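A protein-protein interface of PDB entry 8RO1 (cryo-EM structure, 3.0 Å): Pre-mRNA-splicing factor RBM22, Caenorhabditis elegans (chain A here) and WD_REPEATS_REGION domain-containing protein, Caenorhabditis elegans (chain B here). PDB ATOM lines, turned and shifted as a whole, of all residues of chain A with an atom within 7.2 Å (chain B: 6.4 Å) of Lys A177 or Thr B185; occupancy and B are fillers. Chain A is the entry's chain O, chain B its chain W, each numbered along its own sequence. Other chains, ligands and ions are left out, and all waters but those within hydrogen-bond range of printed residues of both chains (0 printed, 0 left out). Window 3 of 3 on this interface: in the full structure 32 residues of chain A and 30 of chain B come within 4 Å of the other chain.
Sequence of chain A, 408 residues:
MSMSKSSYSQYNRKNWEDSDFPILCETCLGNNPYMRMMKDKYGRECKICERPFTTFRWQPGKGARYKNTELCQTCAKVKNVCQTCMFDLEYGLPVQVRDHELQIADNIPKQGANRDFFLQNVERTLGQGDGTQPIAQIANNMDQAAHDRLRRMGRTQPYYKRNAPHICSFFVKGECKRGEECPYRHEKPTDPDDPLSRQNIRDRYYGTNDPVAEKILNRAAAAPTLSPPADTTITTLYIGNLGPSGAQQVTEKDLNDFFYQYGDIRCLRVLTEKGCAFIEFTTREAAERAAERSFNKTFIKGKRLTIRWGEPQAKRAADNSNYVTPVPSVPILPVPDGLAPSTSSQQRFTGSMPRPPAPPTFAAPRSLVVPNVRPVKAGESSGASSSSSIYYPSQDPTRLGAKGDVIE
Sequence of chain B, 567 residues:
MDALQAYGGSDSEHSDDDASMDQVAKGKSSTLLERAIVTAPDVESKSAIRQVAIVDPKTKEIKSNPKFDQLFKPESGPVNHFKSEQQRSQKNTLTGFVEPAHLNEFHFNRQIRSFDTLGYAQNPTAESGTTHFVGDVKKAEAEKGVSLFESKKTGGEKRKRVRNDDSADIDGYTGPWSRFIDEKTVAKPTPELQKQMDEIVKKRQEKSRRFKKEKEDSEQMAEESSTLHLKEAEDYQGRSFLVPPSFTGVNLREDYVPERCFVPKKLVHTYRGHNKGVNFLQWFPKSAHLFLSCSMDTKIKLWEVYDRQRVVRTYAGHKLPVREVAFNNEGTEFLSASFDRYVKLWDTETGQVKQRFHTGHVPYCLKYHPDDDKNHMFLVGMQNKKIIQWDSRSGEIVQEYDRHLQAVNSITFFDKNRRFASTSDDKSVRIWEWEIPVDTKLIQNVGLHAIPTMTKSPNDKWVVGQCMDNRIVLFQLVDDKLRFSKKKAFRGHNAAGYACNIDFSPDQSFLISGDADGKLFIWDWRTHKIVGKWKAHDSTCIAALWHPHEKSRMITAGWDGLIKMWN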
ATOM      1  N   PHE A 170     -16.447 -14.546 -10.604  1.00  0.00           N
ATOM      2  CA  PHE A 170     -17.790 -13.955 -10.705  1.00  0.00           C
ATOM      3  C   PHE A 170     -18.020 -12.765  -9.792  1.00  0.00           C
ATOM      4  O   PHE A 170     -18.802 -11.876 -10.127  1.00  0.00           O
ATOM      5  CB  PHE A 170     -18.860 -14.974 -10.401  1.00  0.00           C
ATOM      6  CG  PHE A 170     -18.889 -16.093 -11.346  1.00  0.00           C
ATOM      7  CD1 PHE A 170     -19.445 -15.934 -12.586  1.00  0.00           C
ATOM      8  CD2 PHE A 170     -18.247 -17.261 -11.037  1.00  0.00           C
ATOM      9  CE1 PHE A 170     -19.384 -16.943 -13.501  1.00  0.00           C
ATOM     10  CE2 PHE A 170     -18.200 -18.280 -11.911  1.00  0.00           C
ATOM     11  CZ  PHE A 170     -18.782 -18.137 -13.148  1.00  0.00           C
ATOM     12  N   PHE A 171     -17.396 -12.755  -8.618  1.00  0.00           N
ATOM     13  CA  PHE A 171     -17.373 -11.581  -7.764  1.00  0.00           C
ATOM     14  C   PHE A 171     -16.497 -10.483  -8.325  1.00  0.00           C
ATOM     15  O   PHE A 171     -16.788  -9.305  -8.094  1.00  0.00           O
ATOM     16  CB  PHE A 171     -16.902 -11.994  -6.383  1.00  0.00           C
ATOM     17  CG  PHE A 171     -16.801 -10.876  -5.400  1.00  0.00           C
ATOM     18  CD1 PHE A 171     -17.926 -10.388  -4.782  1.00  0.00           C
ATOM     19  CD2 PHE A 171     -15.586 -10.357  -5.049  1.00  0.00           C
ATOM     20  CE1 PHE A 171     -17.836  -9.389  -3.849  1.00  0.00           C
ATOM     21  CE2 PHE A 171     -15.485  -9.355  -4.114  1.00  0.00           C
ATOM     22  CZ  PHE A 171     -16.615  -8.872  -3.508  1.00  0.00           C
ATOM     23  N   GLY A 174     -18.598  -8.999 -10.470  1.00  0.00           N
ATOM     24  CA  GLY A 174     -19.556  -8.375  -9.586  1.00  0.00           C
ATOM     25  C   GLY A 174     -20.933  -9.003  -9.538  1.00  0.00           C
ATOM     26  O   GLY A 174     -21.901  -8.289  -9.264  1.00  0.00           O
ATOM     27  N   GLU A 175     -21.056 -10.309  -9.814  1.00  0.00           N
ATOM     28  CA  GLU A 175     -22.349 -10.927 -10.101  1.00  0.00           C
ATOM     29  C   GLU A 175     -22.490 -12.307  -9.470  1.00  0.00           C
ATOM     30  O   GLU A 175     -23.176 -13.171 -10.017  1.00  0.00           O
ATOM     31  CB  GLU A 175     -22.562 -11.002 -11.616  1.00  0.00           C
ATOM     32  CG  GLU A 175     -21.516 -11.833 -12.376  1.00  0.00           C
ATOM     33  CD  GLU A 175     -22.053 -12.404 -13.664  1.00  0.00           C
ATOM     34  OE1 GLU A 175     -23.057 -13.145 -13.596  1.00  0.00           O
ATOM     35  OE2 GLU A 175     -21.480 -12.112 -14.735  1.00  0.00           O
ATOM     36  N   CYS A 176     -21.830 -12.543  -8.344  1.00  0.00           N
ATOM     37  CA  CYS A 176     -21.754 -13.901  -7.806  1.00  0.00           C
ATOM     38  C   CYS A 176     -23.038 -14.329  -7.098  1.00  0.00           C
ATOM     39  O   CYS A 176     -23.207 -14.087  -5.903  1.00  0.00           O
ATOM     40  CB  CYS A 176     -20.577 -14.075  -6.876  1.00  0.00           C
ATOM     41  SG  CYS A 176     -20.491 -15.807  -6.534  1.00  0.00           S
ATOM     42  N   LYS A 177     -23.966 -14.942  -7.841  1.00  0.00           N
ATOM     43  CA  LYS A 177     -25.243 -15.396  -7.279  1.00  0.00           C
ATOM     44  C   LYS A 177     -25.090 -16.396  -6.131  1.00  0.00           C
ATOM     45  O   LYS A 177     -26.059 -16.616  -5.394  1.00  0.00           O
ATOM     46  CB  LYS A 177     -26.128 -16.028  -8.355  1.00  0.00           C
ATOM     47  CG  LYS A 177     -27.161 -15.099  -9.040  1.00  0.00           C
ATOM     48  CD  LYS A 177     -26.582 -14.126 -10.032  1.00  0.00           C
ATOM     49  CE  LYS A 177     -26.093 -14.854 -11.282  1.00  0.00           C
ATOM     50  NZ  LYS A 177     -25.346 -13.967 -12.193  1.00  0.00           N
ATOM     51  N   ARG A 178     -23.929 -17.023  -5.974  1.00  0.00           N
ATOM     52  CA  ARG A 178     -23.620 -17.914  -4.860  1.00  0.00           C
ATOM     53  C   ARG A 178     -23.350 -17.234  -3.525  1.00  0.00           C
ATOM     54  O   ARG A 178     -23.195 -17.942  -2.530  1.00  0.00           O
ATOM     55  CB  ARG A 178     -22.422 -18.773  -5.207  1.00  0.00           C
ATOM     56  CG  ARG A 178     -22.638 -19.654  -6.381  1.00  0.00           C
ATOM     57  CD  ARG A 178     -21.429 -20.512  -6.590  1.00  0.00           C
ATOM     58  NE  ARG A 178     -21.311 -21.589  -5.627  1.00  0.00           N
ATOM     59  CZ  ARG A 178     -20.340 -22.490  -5.679  1.00  0.00           C
ATOM     60  NH1 ARG A 178     -20.275 -23.499  -4.832  1.00  0.00           N
ATOM     61  NH2 ARG A 178     -19.392 -22.369  -6.606  1.00  0.00           N
ATOM     62  N   GLY A 179     -23.286 -15.911  -3.452  1.00  0.00           N
ATOM     63  CA  GLY A 179     -22.462 -15.188  -2.498  1.00  0.00           C
ATOM     64  C   GLY A 179     -22.211 -15.620  -1.059  1.00  0.00           C
ATOM     65  O   GLY A 179     -21.033 -15.727  -0.716  1.00  0.00           O
ATOM     66  N   GLU A 180     -23.184 -15.947  -0.221  1.00  0.00           N
ATOM     67  CA  GLU A 180     -22.793 -16.492   1.086  1.00  0.00           C
ATOM     68  C   GLU A 180     -22.272 -17.912   0.987  1.00  0.00           C
ATOM     69  O   GLU A 180     -21.389 -18.298   1.755  1.00  0.00           O
ATOM     70  CB  GLU A 180     -23.936 -16.439   2.090  1.00  0.00           C
ATOM     71  CG  GLU A 180     -24.137 -15.074   2.696  1.00  0.00           C
ATOM     72  CD  GLU A 180     -25.113 -15.095   3.849  1.00  0.00           C
ATOM     73  OE1 GLU A 180     -25.001 -15.997   4.705  1.00  0.00           O
ATOM     74  OE2 GLU A 180     -25.968 -14.199   3.922  1.00  0.00           O
ATOM     75  N   GLU A 181     -22.797 -18.692   0.053  1.00  0.00           N
ATOM     76  CA  GLU A 181     -22.472 -20.106  -0.045  1.00  0.00           C
ATOM     77  C   GLU A 181     -21.066 -20.399  -0.573  1.00  0.00           C
ATOM     78  O   GLU A 181     -20.526 -21.433  -0.207  1.00  0.00           O
ATOM     79  CB  GLU A 181     -23.537 -20.787  -0.907  1.00  0.00           C
ATOM     80  CG  GLU A 181     -23.374 -22.299  -1.090  1.00  0.00           C
ATOM     81  CD  GLU A 181     -22.490 -22.725  -2.266  1.00  0.00           C
ATOM     82  OE1 GLU A 181     -22.391 -21.974  -3.255  1.00  0.00           O
ATOM     83  OE2 GLU A 181     -21.876 -23.809  -2.194  1.00  0.00           O
ATOM     84  N   CYS A 182     -20.444 -19.445  -1.301  1.00  0.00           N
ATOM     85  CA  CYS A 182     -19.449 -19.404  -2.398  1.00  0.00           C
ATOM     86  C   CYS A 182     -18.163 -20.255  -2.550  1.00  0.00           C
ATOM     87  O   CYS A 182     -17.622 -20.277  -3.663  1.00  0.00           O
ATOM     88  CB  CYS A 182     -18.963 -17.957  -2.479  1.00  0.00           C
ATOM     89  SG  CYS A 182     -18.460 -17.464  -4.082  1.00  0.00           S
ATOM     90  N   ARG B 179     -32.921 -20.889   3.249  1.00  0.00           N
ATOM     91  CA  ARG B 179     -32.334 -19.579   3.353  1.00  0.00           C
ATOM     92  C   ARG B 179     -32.783 -19.098   4.716  1.00  0.00           C
ATOM     93  O   ARG B 179     -33.755 -19.619   5.265  1.00  0.00           O
ATOM     94  CB  ARG B 179     -32.835 -18.641   2.248  1.00  0.00           C
ATOM     95  CG  ARG B 179     -33.217 -19.261   0.877  1.00  0.00           C
ATOM     96  CD  ARG B 179     -32.248 -20.285   0.280  1.00  0.00           C
ATOM     97  NE  ARG B 179     -30.880 -19.780   0.236  1.00  0.00           N
ATOM     98  CZ  ARG B 179     -29.915 -20.232  -0.555  1.00  0.00           C
ATOM     99  NH1 ARG B 179     -28.686 -19.749  -0.413  1.00  0.00           N
ATOM    100  NH2 ARG B 179     -30.146 -21.126  -1.504  1.00  0.00           N
ATOM    101  N   GLU B 183     -30.426 -13.139   5.230  1.00  0.00           N
ATOM    102  CA  GLU B 183     -29.387 -13.758   4.422  1.00  0.00           C
ATOM    103  C   GLU B 183     -29.081 -12.877   3.218  1.00  0.00           C
ATOM    104  O   GLU B 183     -29.956 -12.174   2.707  1.00  0.00           O
ATOM    105  CB  GLU B 183     -29.829 -15.159   3.984  1.00  0.00           C
ATOM    106  CG  GLU B 183     -28.859 -15.888   3.076  1.00  0.00           C
ATOM    107  CD  GLU B 183     -29.081 -17.388   3.044  1.00  0.00           C
ATOM    108  OE1 GLU B 183     -29.442 -17.978   4.082  1.00  0.00           O
ATOM    109  OE2 GLU B 183     -28.879 -17.988   1.970  1.00  0.00           O
ATOM    110  N   LYS B 184     -27.825 -12.946   2.769  1.00  0.00           N
ATOM    111  CA  LYS B 184     -27.378 -12.462   1.466  1.00  0.00           C
ATOM    112  C   LYS B 184     -27.291 -13.630   0.491  1.00  0.00           C
ATOM    113  O   LYS B 184     -26.472 -14.536   0.667  1.00  0.00           O
ATOM    114  CB  LYS B 184     -26.030 -11.748   1.564  1.00  0.00           C
ATOM    115  CG  LYS B 184     -26.076 -10.358   2.182  1.00  0.00           C
ATOM    116  CD  LYS B 184     -24.708  -9.698   2.133  1.00  0.00           C
ATOM    117  CE  LYS B 184     -24.718  -8.330   2.797  1.00  0.00           C
ATOM    118  NZ  LYS B 184     -25.532  -7.339   2.036  1.00  0.00           N
ATOM    119  N   THR B 185     -28.138 -13.611  -0.528  1.00  0.00           N
ATOM    120  CA  THR B 185     -28.000 -14.575  -1.612  1.00  0.00           C
ATOM    121  C   THR B 185     -26.919 -14.159  -2.601  1.00  0.00           C
ATOM    122  O   THR B 185     -26.310 -15.026  -3.235  1.00  0.00           O
ATOM    123  CB  THR B 185     -29.349 -14.752  -2.322  1.00  0.00           C
ATOM    124  OG1 THR B 185     -29.265 -15.844  -3.243  1.00  0.00           O
ATOM    125  CG2 THR B 185     -29.808 -13.471  -3.070  1.00  0.00           C
ATOM    126  N   VAL B 186     -26.672 -12.855  -2.749  1.00  0.00           N
ATOM    127  CA  VAL B 186     -25.710 -12.332  -3.710  1.00  0.00           C
ATOM    128  C   VAL B 186     -24.953 -11.179  -3.058  1.00  0.00           C
ATOM    129  O   VAL B 186     -25.494 -10.453  -2.218  1.00  0.00           O
ATOM    130  CB  VAL B 186     -26.424 -11.923  -5.027  1.00  0.00           C
ATOM    131  CG1 VAL B 186     -27.420 -10.779  -4.804  1.00  0.00           C
ATOM    132  CG2 VAL B 186     -25.425 -11.583  -6.120  1.00  0.00           C
ATOM    133  N   ALA B 187     -23.690 -11.018  -3.454  1.00  0.00           N
ATOM    134  CA  ALA B 187     -22.773 -10.034  -2.891  1.00  0.00           C
ATOM    135  C   ALA B 187     -22.037  -9.357  -4.035  1.00  0.00           C
ATOM    136  O   ALA B 187     -21.644 -10.030  -4.992  1.00  0.00           O
ATOM    137  CB  ALA B 187     -21.778 -10.685  -1.924  1.00  0.00           C
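O of Thr B185 lies close to O of Lys A177 (2.7 Å).
O of Thr B185 lies within hydrogen-bond range of N of Gly A179.
The side-chain carboxylate of Glu A180 lies within hydrogen-bond range of the backbone NH of Lys B184 (2.5 Å).
The side-chain amino group of Lys A177 lies within salt-bridge range of the side-chain carboxylate of Glu A175, at 2.8 Å.
SG of Cys A176 sits close to N of Arg A178 (3.7 Å).
The side-chain carboxylate (OE1) of Glu A181 lies within salt-bridge range of the guanidinium group (NE) of Arg A178 (2.6 Å).
NH1 of Arg B179 lies within salt-bridge range of OE2 of Glu B183.
Phe A171 touches Ala B187.
Cys A176 touches Val B186.
O of Cys A176 touches N of Ala B187 (3.96 Å).
CA of Lys A177 touches CG2 of Val B186, at 3.99 Å.
Thr B185 touches Arg A178 (O to C, 3.7 Å).
Glu A180 touches Glu B183.
Printed residues of chain B within 4 Å of Lys A177: Thr B185 and Val B186.
Of chain A, only Lys A177, Arg A178 and Gly A179 come within 4 Å of Thr B185.
Of the printed residues of chain B, Cys A176 touches Val B186 (3.4 Å) and Ala B187 (3.96 Å).
Of the printed residues of chain B, Gly A179 touches Thr B185 (3.2 Å).
Of the printed residues of chain A, Ala B187 touches Phe A171 and Cys A176.
Of the printed residues of chain A, Glu B183 touches Glu A180.
Of the printed residues of chain B, Phe A171 touches Ala B187.
The nearest printed residue of chain B that does not touch Lys A177 is Ala B187 (5.9 Å).
The nearest residue of chain A that does not touch Thr B185 is Cys A176 (4.2 Å).
Of the 11 printed residues of chain A, 6 touch a printed residue of chain B.
Hydrophobic or aromatic side chains of chain A that line the printed part of chain B: Phe A171.
Hydrophobic or aromatic side chains of chain B within 4 Å of the printed part of chain A: Val B186.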
